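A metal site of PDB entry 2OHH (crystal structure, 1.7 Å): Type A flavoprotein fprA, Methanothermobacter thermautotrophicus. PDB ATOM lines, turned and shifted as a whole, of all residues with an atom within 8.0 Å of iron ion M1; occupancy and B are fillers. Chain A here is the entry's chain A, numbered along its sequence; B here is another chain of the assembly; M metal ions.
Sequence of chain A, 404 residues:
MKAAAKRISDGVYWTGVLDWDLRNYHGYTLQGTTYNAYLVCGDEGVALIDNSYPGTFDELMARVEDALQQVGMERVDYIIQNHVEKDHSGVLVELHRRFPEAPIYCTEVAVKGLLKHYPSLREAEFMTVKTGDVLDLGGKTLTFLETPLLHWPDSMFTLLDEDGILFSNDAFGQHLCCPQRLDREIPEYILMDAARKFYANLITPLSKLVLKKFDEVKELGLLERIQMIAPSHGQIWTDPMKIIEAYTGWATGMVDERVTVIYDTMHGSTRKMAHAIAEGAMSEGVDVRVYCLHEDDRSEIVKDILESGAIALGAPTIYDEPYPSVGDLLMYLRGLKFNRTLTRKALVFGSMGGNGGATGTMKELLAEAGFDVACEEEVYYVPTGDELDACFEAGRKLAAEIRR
NE2 of His 88 is bound to iron ion M1, at 1.9 Å.
Iron ion M1 is bound by NE2 of His 233 (2.0 Å).
Iron ion M1 is bound by OD1 of Asp 170, 2.1 Å away.
Iron ion M1 is bound by OD2 of Asp 170, at 2.5 Å.
Iron ion M1 has four donor atoms within binding distance.
Slightly farther from iron ion M1 lies OD2 of Asp 87 (2.7 Å).
The side-chain carboxylate (OD2) of Asp 87 sits close to a ring nitrogen (NE2) of His 88 (3.2 Å).
OD2 of Asp 87 sits close to NE2 of His 233 (3.1 Å).
The backbone carbonyl oxygen (O) of Thr 34 lies within hydrogen-bond range of a ring nitrogen (ND1) of His 233, at 2.6 Å.
ND1 of His 233 lies within hydrogen-bond range of OG1 of Thr 33.
The backbone NH of His 233 sits close to the side-chain amide nitrogen of Asn 36 (3.5 Å).
OD2 of Asp 87 sits close to OH of Tyr 25, at 3.2 Å.
Within 4 Å of iron ion M1: Asp 87, His 88, Asp 170 and His 233.
The nearest printed residue that does not touch iron ion M1 is Glu 85 (4.4 Å).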
ATOM      1  N   TYR A  25     -16.502  -8.705  -2.183  1.00  0.00           N
ATOM      2  CA  TYR A  25     -16.871  -9.920  -1.501  1.00  0.00           C
ATOM      3  C   TYR A  25     -15.723 -10.915  -1.638  1.00  0.00           C
ATOM      4  O   TYR A  25     -15.391 -11.324  -2.726  1.00  0.00           O
ATOM      5  CB  TYR A  25     -18.228 -10.451  -2.040  1.00  0.00           C
ATOM      6  CG  TYR A  25     -18.734 -11.626  -1.240  1.00  0.00           C
ATOM      7  CD1 TYR A  25     -18.739 -11.573   0.165  1.00  0.00           C
ATOM      8  CD2 TYR A  25     -19.165 -12.805  -1.878  1.00  0.00           C
ATOM      9  CE1 TYR A  25     -19.165 -12.652   0.926  1.00  0.00           C
ATOM     10  CE2 TYR A  25     -19.589 -13.895  -1.126  1.00  0.00           C
ATOM     11  CZ  TYR A  25     -19.591 -13.808   0.285  1.00  0.00           C
ATOM     12  OH  TYR A  25     -20.014 -14.857   1.079  1.00  0.00           O
ATOM     13  N   HIS A  26     -15.087 -11.251  -0.517  1.00  0.00           N
ATOM     14  CA  HIS A  26     -13.870 -12.041  -0.473  1.00  0.00           C
ATOM     15  C   HIS A  26     -12.867 -11.729  -1.580  1.00  0.00           C
ATOM     16  O   HIS A  26     -12.433 -12.622  -2.342  1.00  0.00           O
ATOM     17  CB  HIS A  26     -14.174 -13.527  -0.324  1.00  0.00           C
ATOM     18  CG  HIS A  26     -14.975 -14.116  -1.437  1.00  0.00           C
ATOM     19  ND1 HIS A  26     -14.477 -14.281  -2.702  1.00  0.00           N
ATOM     20  CD2 HIS A  26     -16.233 -14.626  -1.448  1.00  0.00           C
ATOM     21  CE1 HIS A  26     -15.410 -14.832  -3.476  1.00  0.00           C
ATOM     22  NE2 HIS A  26     -16.474 -15.061  -2.731  1.00  0.00           N
ATOM     23  N   THR A  33     -24.795  -7.915  -5.457  1.00  0.00           N
ATOM     24  CA  THR A  33     -24.997  -9.265  -5.831  1.00  0.00           C
ATOM     25  C   THR A  33     -26.353  -9.581  -5.362  1.00  0.00           C
ATOM     26  O   THR A  33     -27.070  -8.721  -4.860  1.00  0.00           O
ATOM     27  CB  THR A  33     -24.003 -10.244  -5.221  1.00  0.00           C
ATOM     28  OG1 THR A  33     -24.238 -11.499  -5.864  1.00  0.00           O
ATOM     29  CG2 THR A  33     -24.224 -10.394  -3.722  1.00  0.00           C
ATOM     30  N   THR A  34     -26.739 -10.826  -5.532  1.00  0.00           N
ATOM     31  CA  THR A  34     -27.969 -11.235  -4.908  1.00  0.00           C
ATOM     32  C   THR A  34     -27.714 -12.516  -4.129  1.00  0.00           C
ATOM     33  O   THR A  34     -26.711 -13.229  -4.358  1.00  0.00           O
ATOM     34  CB  THR A  34     -29.116 -11.544  -5.891  1.00  0.00           C
ATOM     35  OG1 THR A  34     -28.863 -12.758  -6.567  1.00  0.00           O
ATOM     36  CG2 THR A  34     -29.379 -10.406  -6.861  1.00  0.00           C
ATOM     37  N   TYR A  35     -28.575 -12.770  -3.172  1.00  0.00           N
ATOM     38  CA  TYR A  35     -28.555 -14.057  -2.449  1.00  0.00           C
ATOM     39  C   TYR A  35     -29.858 -14.699  -2.803  1.00  0.00           C
ATOM     40  O   TYR A  35     -30.949 -14.262  -2.335  1.00  0.00           O
ATOM     41  CB  TYR A  35     -28.368 -13.871  -0.925  1.00  0.00           C
ATOM     42  CG  TYR A  35     -27.267 -12.896  -0.628  1.00  0.00           C
ATOM     43  CD1 TYR A  35     -25.956 -13.158  -1.059  1.00  0.00           C
ATOM     44  CD2 TYR A  35     -27.532 -11.705   0.016  1.00  0.00           C
ATOM     45  CE1 TYR A  35     -24.946 -12.266  -0.827  1.00  0.00           C
ATOM     46  CE2 TYR A  35     -26.517 -10.790   0.244  1.00  0.00           C
ATOM     47  CZ  TYR A  35     -25.239 -11.101  -0.164  1.00  0.00           C
ATOM     48  OH  TYR A  35     -24.241 -10.210   0.010  1.00  0.00           O
ATOM     49  N   ASN A  36     -29.748 -15.608  -3.769  1.00  0.00           N
ATOM     50  CA  ASN A  36     -31.014 -16.223  -4.294  1.00  0.00           C
ATOM     51  C   ASN A  36     -31.375 -17.371  -3.391  1.00  0.00           C
ATOM     52  O   ASN A  36     -30.574 -18.331  -3.168  1.00  0.00           O
ATOM     53  CB  ASN A  36     -30.754 -16.750  -5.728  1.00  0.00           C
ATOM     54  CG  ASN A  36     -30.417 -15.643  -6.657  1.00  0.00           C
ATOM     55  OD1 ASN A  36     -30.862 -14.500  -6.463  1.00  0.00           O
ATOM     56  ND2 ASN A  36     -29.684 -15.960  -7.699  1.00  0.00           N
ATOM     57  N   ASP A  50     -31.878 -22.585   0.162  1.00  0.00           N
ATOM     58  CA  ASP A  50     -30.892 -21.582   0.544  1.00  0.00           C
ATOM     59  C   ASP A  50     -31.513 -20.405   1.253  1.00  0.00           C
ATOM     60  O   ASP A  50     -32.742 -20.295   1.414  1.00  0.00           O
ATOM     61  CB  ASP A  50     -30.038 -21.179  -0.638  1.00  0.00           C
ATOM     62  CG  ASP A  50     -29.066 -22.303  -1.024  1.00  0.00           C
ATOM     63  OD1 ASP A  50     -28.807 -23.147  -0.125  1.00  0.00           O
ATOM     64  OD2 ASP A  50     -28.623 -22.336  -2.183  1.00  0.00           O
ATOM     65  N   HIS A  83     -25.500 -25.152   0.708  1.00  0.00           N
ATOM     66  CA  HIS A  83     -24.125 -24.715   1.000  1.00  0.00           C
ATOM     67  C   HIS A  83     -24.140 -23.902   2.287  1.00  0.00           C
ATOM     68  O   HIS A  83     -25.161 -23.344   2.642  1.00  0.00           O
ATOM     69  CB  HIS A  83     -23.682 -23.963  -0.259  1.00  0.00           C
ATOM     70  CG  HIS A  83     -22.418 -23.205  -0.155  1.00  0.00           C
ATOM     71  ND1 HIS A  83     -21.222 -23.759   0.271  1.00  0.00           N
ATOM     72  CD2 HIS A  83     -22.130 -21.942  -0.536  1.00  0.00           C
ATOM     73  CE1 HIS A  83     -20.279 -22.841   0.202  1.00  0.00           C
ATOM     74  NE2 HIS A  83     -20.803 -21.734  -0.295  1.00  0.00           N
ATOM     75  N   GLU A  85     -21.929 -21.469   3.419  1.00  0.00           N
ATOM     76  CA  GLU A  85     -21.336 -20.156   3.457  1.00  0.00           C
ATOM     77  C   GLU A  85     -22.362 -19.170   3.916  1.00  0.00           C
ATOM     78  O   GLU A  85     -23.550 -19.301   3.622  1.00  0.00           O
ATOM     79  CB  GLU A  85     -20.808 -19.777   2.092  1.00  0.00           C
ATOM     80  CG  GLU A  85     -19.720 -18.707   2.212  1.00  0.00           C
ATOM     81  CD  GLU A  85     -19.092 -18.402   0.863  1.00  0.00           C
ATOM     82  OE1 GLU A  85     -18.404 -17.356   0.755  1.00  0.00           O
ATOM     83  OE2 GLU A  85     -19.276 -19.214  -0.087  1.00  0.00           O
ATOM     84  N   LYS A  86     -21.916 -18.156   4.625  1.00  0.00           N
ATOM     85  CA  LYS A  86     -22.892 -17.324   5.348  1.00  0.00           C
ATOM     86  C   LYS A  86     -23.751 -16.427   4.449  1.00  0.00           C
ATOM     87  O   LYS A  86     -24.785 -15.942   4.892  1.00  0.00           O
ATOM     88  CB  LYS A  86     -22.132 -16.502   6.383  1.00  0.00           C
ATOM     89  CG  LYS A  86     -21.282 -15.484   5.726  1.00  0.00           C
ATOM     90  CD  LYS A  86     -20.385 -14.738   6.716  1.00  0.00           C
ATOM     91  CE  LYS A  86     -21.131 -13.876   7.696  1.00  0.00           C
ATOM     92  NZ  LYS A  86     -20.160 -13.318   8.691  1.00  0.00           N
ATOM     93  N   ASP A  87     -23.376 -16.238   3.183  1.00  0.00           N
ATOM     94  CA  ASP A  87     -24.277 -15.506   2.272  1.00  0.00           C
ATOM     95  C   ASP A  87     -25.502 -16.310   1.905  1.00  0.00           C
ATOM     96  O   ASP A  87     -26.447 -15.776   1.344  1.00  0.00           O
ATOM     97  CB  ASP A  87     -23.573 -14.964   1.016  1.00  0.00           C
ATOM     98  CG  ASP A  87     -22.714 -15.992   0.281  1.00  0.00           C
ATOM     99  OD1 ASP A  87     -22.343 -17.092   0.818  1.00  0.00           O
ATOM    100  OD2 ASP A  87     -22.346 -15.691  -0.886  1.00  0.00           O
ATOM    101  N   HIS A  88     -25.487 -17.600   2.239  1.00  0.00           N
ATOM    102  CA  HIS A  88     -26.579 -18.486   1.900  1.00  0.00           C
ATOM    103  C   HIS A  88     -27.168 -19.134   3.114  1.00  0.00           C
ATOM    104  O   HIS A  88     -28.231 -19.698   3.009  1.00  0.00           O
ATOM    105  CB  HIS A  88     -26.081 -19.548   0.902  1.00  0.00           C
ATOM    106  CG  HIS A  88     -25.427 -18.936  -0.294  1.00  0.00           C
ATOM    107  ND1 HIS A  88     -26.107 -18.052  -1.143  1.00  0.00           N
ATOM    108  CD2 HIS A  88     -24.158 -19.016  -0.748  1.00  0.00           C
ATOM    109  CE1 HIS A  88     -25.235 -17.630  -2.057  1.00  0.00           C
ATOM    110  NE2 HIS A  88     -24.066 -18.210  -1.850  1.00  0.00           N
ATOM    111  N   HIS A 151     -18.889 -25.233  -4.615  1.00  0.00           N
ATOM    112  CA  HIS A 151     -17.507 -24.846  -4.404  1.00  0.00           C
ATOM    113  C   HIS A 151     -16.866 -25.204  -3.050  1.00  0.00           C
ATOM    114  O   HIS A 151     -15.720 -24.852  -2.800  1.00  0.00           O
ATOM    115  CB  HIS A 151     -17.289 -23.370  -4.808  1.00  0.00           C
ATOM    116  CG  HIS A 151     -17.440 -22.372  -3.695  1.00  0.00           C
ATOM    117  ND1 HIS A 151     -16.446 -21.482  -3.347  1.00  0.00           N
ATOM    118  CD2 HIS A 151     -18.450 -22.188  -2.809  1.00  0.00           C
ATOM    119  CE1 HIS A 151     -16.843 -20.778  -2.319  1.00  0.00           C
ATOM    120  NE2 HIS A 151     -18.055 -21.178  -1.961  1.00  0.00           N
ATOM    121  N   ASN A 169     -26.671 -23.882  -6.271  1.00  0.00           N
ATOM    122  CA  ASN A 169     -25.811 -23.195  -5.303  1.00  0.00           C
ATOM    123  C   ASN A 169     -24.987 -22.160  -6.084  1.00  0.00           C
ATOM    124  O   ASN A 169     -25.474 -21.546  -7.037  1.00  0.00           O
ATOM    125  CB  ASN A 169     -24.981 -24.193  -4.355  1.00  0.00           C
ATOM    126  CG  ASN A 169     -23.711 -24.979  -5.004  1.00  0.00           C
ATOM    127  OD1 ASN A 169     -22.708 -24.408  -5.468  1.00  0.00           O
ATOM    128  ND2 ASN A 169     -23.758 -26.317  -4.918  1.00  0.00           N
ATOM    129  N   ASP A 170     -23.746 -21.954  -5.694  1.00  0.00           N
ATOM    130  CA  ASP A 170     -22.944 -20.961  -6.359  1.00  0.00           C
ATOM    131  C   ASP A 170     -22.607 -21.284  -7.813  1.00  0.00           C
ATOM    132  O   ASP A 170     -22.394 -20.358  -8.601  1.00  0.00           O
ATOM    133  CB  ASP A 170     -21.658 -20.704  -5.567  1.00  0.00           C
ATOM    134  CG  ASP A 170     -21.826 -19.555  -4.542  1.00  0.00           C
ATOM    135  OD1 ASP A 170     -22.955 -19.258  -4.103  1.00  0.00           O
ATOM    136  OD2 ASP A 170     -20.813 -18.929  -4.163  1.00  0.00           O
ATOM    137  N   ALA A 171     -22.575 -22.567  -8.177  1.00  0.00           N
ATOM    138  CA  ALA A 171     -22.263 -22.944  -9.545  1.00  0.00           C
ATOM    139  C   ALA A 171     -23.217 -22.256 -10.489  1.00  0.00           C
ATOM    140  O   ALA A 171     -24.404 -22.220 -10.221  1.00  0.00           O
ATOM    141  CB  ALA A 171     -22.374 -24.406  -9.743  1.00  0.00           C
ATOM    142  N   GLY A 173     -23.511 -19.321 -10.911  1.00  0.00           N
ATOM    143  CA  GLY A 173     -23.878 -18.030 -10.336  1.00  0.00           C
ATOM    144  C   GLY A 173     -23.211 -16.868 -11.049  1.00  0.00           C
ATOM    145  O   GLY A 173     -22.236 -17.068 -11.798  1.00  0.00           O
ATOM    146  N   HIS A 175     -22.340 -12.556  -9.942  1.00  0.00           N
ATOM    147  CA  HIS A 175     -22.584 -11.497  -8.949  1.00  0.00           C
ATOM    148  C   HIS A 175     -23.134 -10.357  -9.697  1.00  0.00           C
ATOM    149  O   HIS A 175     -22.391  -9.520 -10.248  1.00  0.00           O
ATOM    150  CB  HIS A 175     -21.284 -11.169  -8.167  1.00  0.00           C
ATOM    151  CG  HIS A 175     -20.960 -12.224  -7.151  1.00  0.00           C
ATOM    152  ND1 HIS A 175     -21.859 -12.654  -6.215  1.00  0.00           N
ATOM    153  CD2 HIS A 175     -19.849 -12.973  -6.969  1.00  0.00           C
ATOM    154  CE1 HIS A 175     -21.326 -13.599  -5.474  1.00  0.00           C
ATOM    155  NE2 HIS A 175     -20.081 -13.797  -5.911  1.00  0.00           N
ATOM    156  N   PHE A 198     -17.225 -14.912 -12.424  1.00  0.00           N
ATOM    157  CA  PHE A 198     -17.523 -15.775 -11.354  1.00  0.00           C
ATOM    158  C   PHE A 198     -16.821 -17.079 -11.558  1.00  0.00           C
ATOM    159  O   PHE A 198     -16.212 -17.596 -10.633  1.00  0.00           O
ATOM    160  CB  PHE A 198     -18.969 -16.018 -11.355  1.00  0.00           C
ATOM    161  CG  PHE A 198     -19.498 -16.645 -10.112  1.00  0.00           C
ATOM    162  CD1 PHE A 198     -20.147 -15.866  -9.161  1.00  0.00           C
ATOM    163  CD2 PHE A 198     -19.452 -18.005  -9.929  1.00  0.00           C
ATOM    164  CE1 PHE A 198     -20.730 -16.437  -8.020  1.00  0.00           C
ATOM    165  CE2 PHE A 198     -19.991 -18.603  -8.788  1.00  0.00           C
ATOM    166  CZ  PHE A 198     -20.636 -17.819  -7.830  1.00  0.00           C
ATOM    167  N   LEU A 202     -13.997 -18.204  -8.847  1.00  0.00           N
ATOM    168  CA  LEU A 202     -14.529 -19.202  -7.907  1.00  0.00           C
ATOM    169  C   LEU A 202     -14.453 -20.601  -8.430  1.00  0.00           C
ATOM    170  O   LEU A 202     -14.406 -21.528  -7.625  1.00  0.00           O
ATOM    171  CB  LEU A 202     -15.987 -18.899  -7.589  1.00  0.00           C
ATOM    172  CG  LEU A 202     -16.010 -17.617  -6.743  1.00  0.00           C
ATOM    173  CD1 LEU A 202     -17.417 -17.030  -6.631  1.00  0.00           C
ATOM    174  CD2 LEU A 202     -15.367 -17.924  -5.381  1.00  0.00           C
ATOM    175  N   PRO A 231     -29.151 -20.407  -9.774  1.00  0.00           N
ATOM    176  CA  PRO A 231     -28.011 -20.407  -8.902  1.00  0.00           C
ATOM    177  C   PRO A 231     -28.253 -19.522  -7.680  1.00  0.00           C
ATOM    178  O   PRO A 231     -29.308 -18.864  -7.557  1.00  0.00           O
ATOM    179  CB  PRO A 231     -26.903 -19.823  -9.782  1.00  0.00           C
ATOM    180  CG  PRO A 231     -27.607 -18.860 -10.673  1.00  0.00           C
ATOM    181  CD  PRO A 231     -29.066 -19.391 -10.832  1.00  0.00           C
ATOM    182  N   SER A 232     -27.265 -19.475  -6.789  1.00  0.00           N
ATOM    183  CA  SER A 232     -27.409 -18.756  -5.524  1.00  0.00           C
ATOM    184  C   SER A 232     -27.069 -17.270  -5.617  1.00  0.00           C
ATOM    185  O   SER A 232     -27.368 -16.495  -4.691  1.00  0.00           O
ATOM    186  CB  SER A 232     -26.578 -19.446  -4.421  1.00  0.00           C
ATOM    187  OG  SER A 232     -27.225 -20.656  -4.049  1.00  0.00           O
ATOM    188  N   HIS A 233     -26.459 -16.868  -6.733  1.00  0.00           N
ATOM    189  CA  HIS A 233     -26.241 -15.473  -7.079  1.00  0.00           C
ATOM    190  C   HIS A 233     -26.628 -15.138  -8.490  1.00  0.00           C
ATOM    191  O   HIS A 233     -26.362 -15.903  -9.426  1.00  0.00           O
ATOM    192  CB  HIS A 233     -24.747 -15.079  -6.917  1.00  0.00           C
ATOM    193  CG  HIS A 233     -24.204 -15.393  -5.578  1.00  0.00           C
ATOM    194  ND1 HIS A 233     -24.518 -14.658  -4.449  1.00  0.00           N
ATOM    195  CD2 HIS A 233     -23.450 -16.430  -5.164  1.00  0.00           C
ATOM    196  CE1 HIS A 233     -23.926 -15.213  -3.399  1.00  0.00           C
ATOM    197  NE2 HIS A 233     -23.253 -16.267  -3.817  1.00  0.00           N
ATOM    198  N   HIS B 267     -14.940 -13.516   6.048  1.00  0.00           N
ATOM    199  CA  HIS B 267     -16.232 -13.567   6.760  1.00  0.00           C
ATOM    200  C   HIS B 267     -16.145 -13.174   8.204  1.00  0.00           C
ATOM    201  O   HIS B 267     -17.123 -13.207   8.942  1.00  0.00           O
ATOM    202  CB  HIS B 267     -16.845 -14.959   6.673  1.00  0.00           C
ATOM    203  CG  HIS B 267     -17.235 -15.344   5.287  1.00  0.00           C
ATOM    204  ND1 HIS B 267     -16.822 -16.524   4.699  1.00  0.00           N
ATOM    205  CD2 HIS B 267     -17.952 -14.683   4.351  1.00  0.00           C
ATOM    206  CE1 HIS B 267     -17.312 -16.583   3.470  1.00  0.00           C
ATOM    207  NE2 HIS B 267     -18.021 -15.487   3.243  1.00  0.00           N
HETATM  208 FE    FE M   1     -22.441 -17.746  -2.693  1.00  0.00          FE
HETATM  209 FE    FE M   2     -19.942 -20.141  -1.636  1.00  0.00          FE
